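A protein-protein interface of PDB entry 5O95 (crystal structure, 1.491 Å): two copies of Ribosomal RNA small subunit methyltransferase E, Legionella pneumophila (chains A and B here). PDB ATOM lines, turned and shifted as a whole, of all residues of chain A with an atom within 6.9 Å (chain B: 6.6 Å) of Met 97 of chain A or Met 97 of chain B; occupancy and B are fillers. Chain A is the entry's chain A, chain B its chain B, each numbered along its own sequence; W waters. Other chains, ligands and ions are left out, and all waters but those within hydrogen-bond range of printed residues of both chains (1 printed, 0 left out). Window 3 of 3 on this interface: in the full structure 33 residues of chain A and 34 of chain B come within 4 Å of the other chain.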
ATOM      1  N   ARG A  94     -16.567  -4.721  -8.833  1.00  0.00           N
ATOM      2  CA  ARG A  94     -18.024  -4.628  -8.707  1.00  0.00           C
ATOM      3  C   ARG A  94     -18.544  -5.759  -7.823  1.00  0.00           C
ATOM      4  O   ARG A  94     -18.996  -6.816  -8.284  1.00  0.00           O
ATOM      5  CB  ARG A  94     -18.673  -4.615 -10.086  1.00  0.00           C
ATOM      6  CG  ARG A  94     -20.196  -4.610 -10.086  1.00  0.00           C
ATOM      7  CD  ARG A  94     -20.792  -3.616  -9.107  1.00  0.00           C
ATOM      8  NE  ARG A  94     -20.429  -2.241  -9.437  1.00  0.00           N
ATOM      9  CZ  ARG A  94     -20.909  -1.174  -8.808  1.00  0.00           C
ATOM     10  NH1 ARG A  94     -21.777  -1.322  -7.816  1.00  0.00           N
ATOM     11  NH2 ARG A  94     -20.525   0.039  -9.174  1.00  0.00           N
ATOM     12  N   MET A  95     -18.507  -5.506  -6.514  1.00  0.00           N
ATOM     13  CA  MET A  95     -18.945  -6.520  -5.563  1.00  0.00           C
ATOM     14  C   MET A  95     -20.441  -6.774  -5.671  1.00  0.00           C
ATOM     15  O   MET A  95     -20.894  -7.902  -5.443  1.00  0.00           O
ATOM     16  CB  MET A  95     -18.564  -6.105  -4.142  1.00  0.00           C
ATOM     17  CG  MET A  95     -18.786  -7.188  -3.096  1.00  0.00           C
ATOM     18  SD  MET A  95     -17.795  -8.671  -3.388  1.00  0.00           S
ATOM     19  CE  MET A  95     -16.197  -7.934  -3.702  1.00  0.00           C
ATOM     20  N   GLU A  96     -21.214  -5.749  -6.043  1.00  0.00           N
ATOM     21  CA  GLU A  96     -22.655  -5.929  -6.185  1.00  0.00           C
ATOM     22  C   GLU A  96     -22.976  -6.946  -7.274  1.00  0.00           C
ATOM     23  O   GLU A  96     -23.901  -7.759  -7.123  1.00  0.00           O
ATOM     24  CB  GLU A  96     -23.330  -4.584  -6.465  1.00  0.00           C
ATOM     25  CG  GLU A  96     -23.243  -3.575  -5.313  1.00  0.00           C
ATOM     26  CD  GLU A  96     -21.828  -3.060  -5.048  1.00  0.00           C
ATOM     27  OE1 GLU A  96     -21.018  -2.982  -6.000  1.00  0.00           O
ATOM     28  OE2 GLU A  96     -21.526  -2.743  -3.877  1.00  0.00           O
ATOM     29  N   MET A  97     -22.213  -6.928  -8.375  1.00  0.00           N
ATOM     30  CA  MET A  97     -22.435  -7.924  -9.417  1.00  0.00           C
ATOM     31  C   MET A  97     -22.067  -9.315  -8.932  1.00  0.00           C
ATOM     32  O   MET A  97     -22.766 -10.278  -9.248  1.00  0.00           O
ATOM     33  CB  MET A  97     -21.651  -7.598 -10.688  1.00  0.00           C
ATOM     34  CG  MET A  97     -21.987  -8.528 -11.826  1.00  0.00           C
ATOM     35  SD  MET A  97     -21.047  -8.231 -13.326  1.00  0.00           S
ATOM     36  CE  MET A  97     -21.718  -9.540 -14.318  1.00  0.00           C
ATOM     37  N   VAL A  98     -20.956  -9.449  -8.199  1.00  0.00           N
ATOM     38  CA  VAL A  98     -20.578 -10.762  -7.673  1.00  0.00           C
ATOM     39  C   VAL A  98     -21.670 -11.318  -6.770  1.00  0.00           C
ATOM     40  O   VAL A  98     -22.014 -12.501  -6.857  1.00  0.00           O
ATOM     41  CB  VAL A  98     -19.234 -10.709  -6.934  1.00  0.00           C
ATOM     42  CG1 VAL A  98     -18.927 -12.064  -6.294  1.00  0.00           C
ATOM     43  CG2 VAL A  98     -18.100 -10.288  -7.890  1.00  0.00           C
ATOM     44  N   MET A  99     -22.208 -10.479  -5.871  1.00  0.00           N
ATOM     45  CA  MET A  99     -23.276 -10.914  -4.970  1.00  0.00           C
ATOM     46  C   MET A  99     -24.480 -11.428  -5.748  1.00  0.00           C
ATOM     47  O   MET A  99     -25.008 -12.506  -5.461  1.00  0.00           O
ATOM     48  CB  MET A  99     -23.678  -9.745  -4.068  1.00  0.00           C
ATOM     49  CG  MET A  99     -22.565  -9.314  -3.117  1.00  0.00           C
ATOM     50  SD  MET A  99     -22.254 -10.591  -1.874  1.00  0.00           S
ATOM     51  CE  MET A  99     -20.658 -10.048  -1.250  1.00  0.00           C
ATOM     52  N   GLN A 100     -24.918 -10.670  -6.755  1.00  0.00           N
ATOM     53  CA  GLN A 100     -26.082 -11.083  -7.528  1.00  0.00           C
ATOM     54  C   GLN A 100     -25.804 -12.359  -8.318  1.00  0.00           C
ATOM     55  O   GLN A 100     -26.585 -13.316  -8.271  1.00  0.00           O
ATOM     56  CB  GLN A 100     -26.470  -9.955  -8.492  1.00  0.00           C
ATOM     57  CG  GLN A 100     -27.718 -10.294  -9.257  1.00  0.00           C
ATOM     58  CD  GLN A 100     -28.066  -9.252 -10.301  1.00  0.00           C
ATOM     59  OE1 GLN A 100     -27.477  -9.223 -11.381  1.00  0.00           O
ATOM     60  NE2 GLN A 100     -29.046  -8.398  -9.989  1.00  0.00           N
ATOM     61  N   LYS A 101     -24.700 -12.381  -9.084  1.00  0.00           N
ATOM     62  CA  LYS A 101     -24.479 -13.509  -9.981  1.00  0.00           C
ATOM     63  C   LYS A 101     -24.060 -14.770  -9.226  1.00  0.00           C
ATOM     64  O   LYS A 101     -24.381 -15.883  -9.655  1.00  0.00           O
ATOM     65  CB  LYS A 101     -23.401 -13.166 -11.029  1.00  0.00           C
ATOM     66  CG  LYS A 101     -23.612 -11.878 -11.809  1.00  0.00           C
ATOM     67  CD  LYS A 101     -25.013 -11.739 -12.312  1.00  0.00           C
ATOM     68  CE  LYS A 101     -25.097 -10.684 -13.419  1.00  0.00           C
ATOM     69  NZ  LYS A 101     -26.529 -10.479 -13.775  1.00  0.00           N
ATOM     70  N   SER A 102     -23.338 -14.633  -8.110  1.00  0.00           N
ATOM     71  CA  SER A 102     -22.951 -15.838  -7.374  1.00  0.00           C
ATOM     72  C   SER A 102     -24.176 -16.492  -6.788  1.00  0.00           C
ATOM     73  O   SER A 102     -24.277 -17.722  -6.749  1.00  0.00           O
ATOM     74  CB  SER A 102     -21.942 -15.524  -6.280  1.00  0.00           C
ATOM     75  OG  SER A 102     -22.482 -14.728  -5.254  1.00  0.00           O
ATOM     76  N   ALA A 103     -25.157 -15.676  -6.407  1.00  0.00           N
ATOM     77  CA  ALA A 103     -26.408 -16.239  -5.904  1.00  0.00           C
ATOM     78  C   ALA A 103     -27.141 -16.977  -7.026  1.00  0.00           C
ATOM     79  O   ALA A 103     -27.647 -18.095  -6.822  1.00  0.00           O
ATOM     80  CB  ALA A 103     -27.260 -15.113  -5.314  1.00  0.00           C
ATOM     81  N   GLU A 104     -27.239 -16.353  -8.206  1.00  0.00           N
ATOM     82  CA  GLU A 104     -27.831 -17.032  -9.355  1.00  0.00           C
ATOM     83  C   GLU A 104     -27.131 -18.344  -9.655  1.00  0.00           C
ATOM     84  O   GLU A 104     -27.760 -19.307 -10.096  1.00  0.00           O
ATOM     85  CB  GLU A 104     -27.743 -16.144 -10.605  1.00  0.00           C
ATOM     86  CG  GLU A 104     -28.593 -14.924 -10.546  1.00  0.00           C
ATOM     87  CD  GLU A 104     -28.507 -14.114 -11.833  1.00  0.00           C
ATOM     88  OE1 GLU A 104     -28.609 -14.718 -12.925  1.00  0.00           O
ATOM     89  OE2 GLU A 104     -28.326 -12.888 -11.730  1.00  0.00           O
ATOM     90  N   ILE A 137     -29.164  -7.609  -2.146  1.00  0.00           N
ATOM     91  CA  ILE A 137     -28.947  -8.032  -3.527  1.00  0.00           C
ATOM     92  C   ILE A 137     -29.066  -9.542  -3.648  1.00  0.00           C
ATOM     93  O   ILE A 137     -29.652 -10.057  -4.606  1.00  0.00           O
ATOM     94  CB  ILE A 137     -27.574  -7.529  -4.012  1.00  0.00           C
ATOM     95  CG1 ILE A 137     -27.600  -6.008  -4.195  1.00  0.00           C
ATOM     96  CG2 ILE A 137     -27.162  -8.232  -5.309  1.00  0.00           C
ATOM     97  CD1 ILE A 137     -26.206  -5.420  -4.437  1.00  0.00           C
ATOM     98  N   GLU A 228     -14.874  -9.618 -11.270  1.00  0.00           N
ATOM     99  CA  GLU A 228     -16.263 -10.056 -11.251  1.00  0.00           C
ATOM    100  C   GLU A 228     -16.538 -11.106 -12.321  1.00  0.00           C
ATOM    101  O   GLU A 228     -17.335 -12.024 -12.106  1.00  0.00           O
ATOM    102  CB  GLU A 228     -17.205  -8.848 -11.368  1.00  0.00           C
ATOM    103  CG  GLU A 228     -17.336  -8.225 -12.758  1.00  0.00           C
ATOM    104  CD  GLU A 228     -16.256  -7.192 -13.096  1.00  0.00           C
ATOM    105  OE1 GLU A 228     -15.300  -7.002 -12.304  1.00  0.00           O
ATOM    106  OE2 GLU A 228     -16.374  -6.561 -14.172  1.00  0.00           O
ATOM    107  N   THR A 229     -15.881 -11.004 -13.473  1.00  0.00           N
ATOM    108  CA  THR A 229     -15.990 -12.070 -14.453  1.00  0.00           C
ATOM    109  C   THR A 229     -15.412 -13.373 -13.907  1.00  0.00           C
ATOM    110  O   THR A 229     -15.944 -14.456 -14.170  1.00  0.00           O
ATOM    111  CB  THR A 229     -15.216 -11.660 -15.704  1.00  0.00           C
ATOM    112  OG1 THR A 229     -15.621 -10.353 -16.094  1.00  0.00           O
ATOM    113  CG2 THR A 229     -15.462 -12.660 -16.860  1.00  0.00           C
ATOM    114  N   ILE A 232     -18.002 -15.234 -11.811  1.00  0.00           N
ATOM    115  CA  ILE A 232     -19.004 -15.890 -12.658  1.00  0.00           C
ATOM    116  C   ILE A 232     -18.412 -17.122 -13.316  1.00  0.00           C
ATOM    117  O   ILE A 232     -19.014 -18.203 -13.332  1.00  0.00           O
ATOM    118  CB  ILE A 232     -19.500 -14.924 -13.752  1.00  0.00           C
ATOM    119  CG1 ILE A 232     -20.085 -13.639 -13.187  1.00  0.00           C
ATOM    120  CG2 ILE A 232     -20.476 -15.638 -14.691  1.00  0.00           C
ATOM    121  CD1 ILE A 232     -20.422 -12.654 -14.303  1.00  0.00           C
ATOM    122  N   GLU B  93     -28.853  -1.891 -20.000  1.00  0.00           N
ATOM    123  CA  GLU B  93     -27.485  -1.982 -20.502  1.00  0.00           C
ATOM    124  C   GLU B  93     -26.923  -3.398 -20.371  1.00  0.00           C
ATOM    125  O   GLU B  93     -25.708  -3.602 -20.282  1.00  0.00           O
ATOM    126  CB  GLU B  93     -26.588  -0.933 -19.852  1.00  0.00           C
ATOM    127  CG  GLU B  93     -26.908   0.488 -20.300  1.00  0.00           C
ATOM    128  CD  GLU B  93     -25.799   1.470 -19.972  1.00  0.00           C
ATOM    129  OE1 GLU B  93     -25.111   1.277 -18.947  1.00  0.00           O
ATOM    130  OE2 GLU B  93     -25.609   2.430 -20.745  1.00  0.00           O
ATOM    131  N   ARG B  94     -27.804  -4.396 -20.410  1.00  0.00           N
ATOM    132  CA  ARG B  94     -27.356  -5.781 -20.307  1.00  0.00           C
ATOM    133  C   ARG B  94     -26.457  -6.164 -21.476  1.00  0.00           C
ATOM    134  O   ARG B  94     -25.474  -6.901 -21.299  1.00  0.00           O
ATOM    135  CB  ARG B  94     -28.581  -6.700 -20.222  1.00  0.00           C
ATOM    136  CG  ARG B  94     -29.398  -6.509 -18.959  1.00  0.00           C
ATOM    137  CD  ARG B  94     -30.829  -6.981 -19.148  1.00  0.00           C
ATOM    138  NE  ARG B  94     -31.592  -6.951 -17.897  1.00  0.00           N
ATOM    139  CZ  ARG B  94     -32.137  -5.855 -17.379  1.00  0.00           C
ATOM    140  NH1 ARG B  94     -32.810  -5.922 -16.236  1.00  0.00           N
ATOM    141  NH2 ARG B  94     -32.003  -4.688 -18.002  1.00  0.00           N
ATOM    142  N   MET B  95     -26.739  -5.638 -22.675  1.00  0.00           N
ATOM    143  CA  MET B  95     -25.922  -6.017 -23.820  1.00  0.00           C
ATOM    144  C   MET B  95     -24.509  -5.497 -23.666  1.00  0.00           C
ATOM    145  O   MET B  95     -23.550  -6.173 -24.055  1.00  0.00           O
ATOM    146  CB  MET B  95     -26.519  -5.478 -25.113  1.00  0.00           C
ATOM    147  CG  MET B  95     -25.833  -5.997 -26.362  1.00  0.00           C
ATOM    148  SD  MET B  95     -25.997  -7.787 -26.582  1.00  0.00           S
ATOM    149  CE  MET B  95     -27.331  -7.817 -27.789  1.00  0.00           C
ATOM    150  N   GLU B  96     -24.356  -4.313 -23.070  1.00  0.00           N
ATOM    151  CA  GLU B  96     -23.009  -3.766 -22.899  1.00  0.00           C
ATOM    152  C   GLU B  96     -22.177  -4.676 -22.008  1.00  0.00           C
ATOM    153  O   GLU B  96     -20.988  -4.895 -22.259  1.00  0.00           O
ATOM    154  CB  GLU B  96     -23.106  -2.357 -22.318  1.00  0.00           C
ATOM    155  CG  GLU B  96     -23.566  -1.267 -23.326  1.00  0.00           C
ATOM    156  CD  GLU B  96     -25.020  -1.346 -23.804  1.00  0.00           C
ATOM    157  OE1 GLU B  96     -25.867  -2.027 -23.185  1.00  0.00           O
ATOM    158  OE2 GLU B  96     -25.331  -0.677 -24.816  1.00  0.00           O
ATOM    159  N   MET B  97     -22.796  -5.257 -20.990  1.00  0.00           N
ATOM    160  CA  MET B  97     -22.099  -6.208 -20.135  1.00  0.00           C
ATOM    161  C   MET B  97     -21.730  -7.464 -20.911  1.00  0.00           C
ATOM    162  O   MET B  97     -20.594  -7.958 -20.803  1.00  0.00           O
ATOM    163  CB  MET B  97     -23.013  -6.535 -18.946  1.00  0.00           C
ATOM    164  CG  MET B  97     -22.289  -6.998 -17.717  1.00  0.00           C
ATOM    165  SD  MET B  97     -23.013  -8.533 -17.172  1.00  0.00           S
ATOM    166  CE  MET B  97     -22.528  -9.567 -18.531  1.00  0.00           C
ATOM    167  N   VAL B  98     -22.656  -7.972 -21.727  1.00  0.00           N
ATOM    168  CA  VAL B  98     -22.394  -9.174 -22.515  1.00  0.00           C
ATOM    169  C   VAL B  98     -21.257  -8.943 -23.495  1.00  0.00           C
ATOM    170  O   VAL B  98     -20.422  -9.823 -23.697  1.00  0.00           O
ATOM    171  CB  VAL B  98     -23.665  -9.644 -23.241  1.00  0.00           C
ATOM    172  CG1 VAL B  98     -23.350 -10.758 -24.204  1.00  0.00           C
ATOM    173  CG2 VAL B  98     -24.709 -10.113 -22.222  1.00  0.00           C
ATOM    174  N   MET B  99     -21.254  -7.786 -24.174  1.00  0.00           N
ATOM    175  CA  MET B  99     -20.157  -7.459 -25.076  1.00  0.00           C
ATOM    176  C   MET B  99     -18.821  -7.526 -24.352  1.00  0.00           C
ATOM    177  O   MET B  99     -17.852  -8.103 -24.867  1.00  0.00           O
ATOM    178  CB  MET B  99     -20.364  -6.061 -25.663  1.00  0.00           C
ATOM    179  CG  MET B  99     -21.559  -5.948 -26.607  1.00  0.00           C
ATOM    180  SD  MET B  99     -21.293  -6.834 -28.153  1.00  0.00           S
ATOM    181  CE  MET B  99     -22.989  -6.900 -28.769  1.00  0.00           C
ATOM    182  N   GLN B 100     -18.723  -6.897 -23.180  1.00  0.00           N
ATOM    183  CA  GLN B 100     -17.438  -6.863 -22.476  1.00  0.00           C
ATOM    184  C   GLN B 100     -17.022  -8.254 -22.010  1.00  0.00           C
ATOM    185  O   GLN B 100     -15.889  -8.701 -22.258  1.00  0.00           O
ATOM    186  CB  GLN B 100     -17.521  -5.894 -21.296  1.00  0.00           C
ATOM    187  CG  GLN B 100     -16.276  -5.897 -20.431  1.00  0.00           C
ATOM    188  CD  GLN B 100     -16.388  -4.974 -19.242  1.00  0.00           C
ATOM    189  OE1 GLN B 100     -16.824  -5.383 -18.166  1.00  0.00           O
ATOM    190  NE2 GLN B 100     -15.988  -3.718 -19.426  1.00  0.00           N
ATOM    191  N   LYS B 101     -17.919  -8.959 -21.337  1.00  0.00           N
ATOM    192  CA  LYS B 101     -17.539 -10.221 -20.732  1.00  0.00           C
ATOM    193  C   LYS B 101     -17.396 -11.344 -21.754  1.00  0.00           C
ATOM    194  O   LYS B 101     -16.611 -12.273 -21.514  1.00  0.00           O
ATOM    195  CB  LYS B 101     -18.540 -10.554 -19.622  1.00  0.00           C
ATOM    196  CG  LYS B 101     -18.447  -9.492 -18.485  1.00  0.00           C
ATOM    197  CD  LYS B 101     -19.014  -9.909 -17.167  1.00  0.00           C
ATOM    198  CE  LYS B 101     -18.796  -8.773 -16.168  1.00  0.00           C
ATOM    199  NZ  LYS B 101     -17.426  -8.178 -16.291  1.00  0.00           N
ATOM    200  N   SER B 102     -18.144 -11.309 -22.862  1.00  0.00           N
ATOM    201  CA  SER B 102     -17.972 -12.368 -23.848  1.00  0.00           C
ATOM    202  C   SER B 102     -16.608 -12.248 -24.517  1.00  0.00           C
ATOM    203  O   SER B 102     -15.959 -13.258 -24.804  1.00  0.00           O
ATOM    204  CB  SER B 102     -19.107 -12.370 -24.867  1.00  0.00           C
ATOM    205  OG  SER B 102     -19.080 -11.204 -25.668  1.00  0.00           O
ATOM    206  N   GLU B 104     -13.901 -11.119 -22.936  1.00  0.00           N
ATOM    207  CA  GLU B 104     -12.987 -11.702 -21.943  1.00  0.00           C
ATOM    208  C   GLU B 104     -13.006 -13.220 -21.994  1.00  0.00           C
ATOM    209  O   GLU B 104     -11.968 -13.869 -21.767  1.00  0.00           O
ATOM    210  CB  GLU B 104     -13.362 -11.265 -20.520  1.00  0.00           C
ATOM    211  CG  GLU B 104     -13.204  -9.797 -20.244  1.00  0.00           C
ATOM    212  CD  GLU B 104     -13.724  -9.401 -18.859  1.00  0.00           C
ATOM    213  OE1 GLU B 104     -13.392 -10.073 -17.865  1.00  0.00           O
ATOM    214  OE2 GLU B 104     -14.468  -8.404 -18.773  1.00  0.00           O
ATOM    215  N   ILE B 137     -16.594  -1.186 -26.787  1.00  0.00           N
ATOM    216  CA  ILE B 137     -16.542  -1.979 -25.557  1.00  0.00           C
ATOM    217  C   ILE B 137     -15.747  -3.259 -25.764  1.00  0.00           C
ATOM    218  O   ILE B 137     -14.969  -3.675 -24.891  1.00  0.00           O
ATOM    219  CB  ILE B 137     -17.974  -2.266 -25.093  1.00  0.00           C
ATOM    220  CG1 ILE B 137     -18.572  -0.980 -24.577  1.00  0.00           C
ATOM    221  CG2 ILE B 137     -18.004  -3.352 -24.012  1.00  0.00           C
ATOM    222  CD1 ILE B 137     -20.098  -1.053 -24.404  1.00  0.00           C
ATOM    223  N   GLU B 228     -27.914 -11.883 -19.187  1.00  0.00           N
ATOM    224  CA  GLU B 228     -26.492 -11.575 -19.229  1.00  0.00           C
ATOM    225  C   GLU B 228     -25.696 -12.590 -18.435  1.00  0.00           C
ATOM    226  O   GLU B 228     -24.586 -12.949 -18.835  1.00  0.00           O
ATOM    227  CB  GLU B 228     -26.208 -10.139 -18.769  1.00  0.00           C
ATOM    228  CG  GLU B 228     -26.321  -9.868 -17.279  1.00  0.00           C
ATOM    229  CD  GLU B 228     -27.742  -9.581 -16.810  1.00  0.00           C
ATOM    230  OE1 GLU B 228     -28.692  -9.758 -17.594  1.00  0.00           O
ATOM    231  OE2 GLU B 228     -27.899  -9.169 -15.644  1.00  0.00           O
ATOM    232  N   THR B 229     -26.260 -13.106 -17.340  1.00  0.00           N
ATOM    233  CA  THR B 229     -25.561 -14.168 -16.627  1.00  0.00           C
ATOM    234  C   THR B 229     -25.473 -15.408 -17.492  1.00  0.00           C
ATOM    235  O   THR B 229     -24.433 -16.076 -17.528  1.00  0.00           O
ATOM    236  CB  THR B 229     -26.337 -14.503 -15.356  1.00  0.00           C
ATOM    237  OG1 THR B 229     -26.556 -13.315 -14.601  1.00  0.00           O
ATOM    238  CG2 THR B 229     -25.522 -15.490 -14.497  1.00  0.00           C
ATOM    239  N   ALA B 231     -25.395 -15.770 -20.767  1.00  0.00           N
ATOM    240  CA  ALA B 231     -24.343 -15.659 -21.770  1.00  0.00           C
ATOM    241  C   ALA B 231     -22.988 -16.002 -21.186  1.00  0.00           C
ATOM    242  O   ALA B 231     -22.231 -16.785 -21.767  1.00  0.00           O
ATOM    243  CB  ALA B 231     -24.317 -14.245 -22.346  1.00  0.00           C
ATOM    244  N   ILE B 232     -22.647 -15.394 -20.054  1.00  0.00           N
ATOM    245  CA  ILE B 232     -21.288 -15.581 -19.555  1.00  0.00           C
ATOM    246  C   ILE B 232     -21.120 -16.972 -18.943  1.00  0.00           C
ATOM    247  O   ILE B 232     -20.056 -17.581 -19.054  1.00  0.00           O
ATOM    248  CB  ILE B 232     -20.885 -14.422 -18.628  1.00  0.00           C
ATOM    249  CG1 ILE B 232     -21.137 -13.076 -19.334  1.00  0.00           C
ATOM    250  CG2 ILE B 232     -19.389 -14.504 -18.285  1.00  0.00           C
ATOM    251  CD1 ILE B 232     -20.747 -13.032 -20.852  1.00  0.00           C
HETATM  252  O   HOH W   1     -16.374  -3.864 -15.431  1.00  0.00           O
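OE2 of Glu 228 of chain B is in salt-bridge range of NZ of Lys 101 of chain A (2.7 Å). The side-chain amino group (NZ) of Lys 101 of chain A is in hydrogen-bond range of the side-chain hydroxyl (OG1) of Thr 229 of chain B (3.0 Å). OG1 of Thr 229 of chain B sits at hydrogen-bond distance from OE1 of Glu 104 of chain A, 3.0 Å away. The side-chain carboxylate (OE2) of Glu 228 of chain A is in salt-bridge range of the side-chain amino group (NZ) of Lys 101 of chain B, 2.9 Å away. The side-chain hydroxyl of Thr 229 of chain A lies within hydrogen-bond range of the side-chain amino group of Lys 101 of chain B (2.8 Å). OE1 of Glu 104 of chain B is in hydrogen-bond range of OG1 of Thr 229 of chain A (2.9 Å).
The side-chain amino group of Lys 101 of chain A lies within hydrogen-bond range of the side-chain amide oxygen of Gln 100 of chain A (2.9 Å). The side-chain carboxylate of Glu 104 of chain A lies within salt-bridge range of the side-chain amino group of Lys 101 of chain A (3.6 Å). The side-chain amino group (NZ) of Lys 101 of chain B lies within hydrogen-bond range of the side-chain amide oxygen (OE1) of Gln 100 of chain B (3.4 Å). OE2 of Glu 104 of chain B is in salt-bridge range of NZ of Lys 101 of chain B.
Among the printed residues, merely in contact across the chains: Met 97 of chain A with Met 97 of chain B (3.3 Å), Met 97 of chain A with Lys 101 of chain B (3.5 Å) and Ile 232 of chain A with Ile 232 of chain B (3.9 Å).
Of chain B, only Met 97 and Lys 101 come within 4 Å of Met 97 of chain A. Met 97 of chain B touches just one residue of chain A: Met 97. Printed residues of chain A within 4 Å of Thr 229 of chain B: Lys 101 (3.0 Å) and Glu 104 (3.0 Å). Of the printed residues of chain A, Glu 104 of chain B touches Thr 229. Of the printed residues of chain A, Glu 228 of chain B touches Lys 101 (2.7 Å). Printed residues of chain B within 4 Å of Glu 228 of chain A: Lys 101 (2.9 Å). Of the printed residues of chain B, Glu 104 of chain A touches Thr 229. Glu 96 of chain A touches none of the printed residues of chain B. Glu 96 of chain B touches none of the printed residues of chain A. The nearest residue of chain B that does not touch Met 97 of chain A is Glu 228 of chain B (5.5 Å). The nearest residue of chain A that does not touch Met 97 of chain B is Lys 101 of chain A (4.8 Å).
Of the 16 printed residues of chain B, 6 touch a printed residue of chain A. Hydrophobic or aromatic side chains of chain B within 4 Å of the printed part of chain A: Met 97 and Ile 232. Printed residues of chain A that touch a printed residue of chain B: Met 97, Lys 101, Glu 104, Glu 228, Thr 229 and Ile 232. Hydrophobic or aromatic side chains of chain A that line the printed part of chain B: Met 97 and Ile 232. Along chain A the printed residues that touch a printed residue of chain B span positions 97 to 232.
Met 97 of chain A touches Lys 101 of chain B, but with the chains exchanged Lys 101 of chain A does not touch Met 97 of chain B (4.8 Å). Lys 101 of chain A touches Glu 228 of chain B, and with the chains exchanged Glu 228 of chain A touches Lys 101 of chain B. Glu 104 of chain A touches Thr 229 of chain B, and with the chains exchanged Thr 229 of chain A touches Glu 104 of chain B. Ile 232 of chain A touches its own counterpart, Ile 232 of chain B. 14 positions are printed for both chains.
Water W1 lies within hydrogen-bond range of OE2 of Glu 228 of chain A and OE1 of Gln 100 of chain B.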
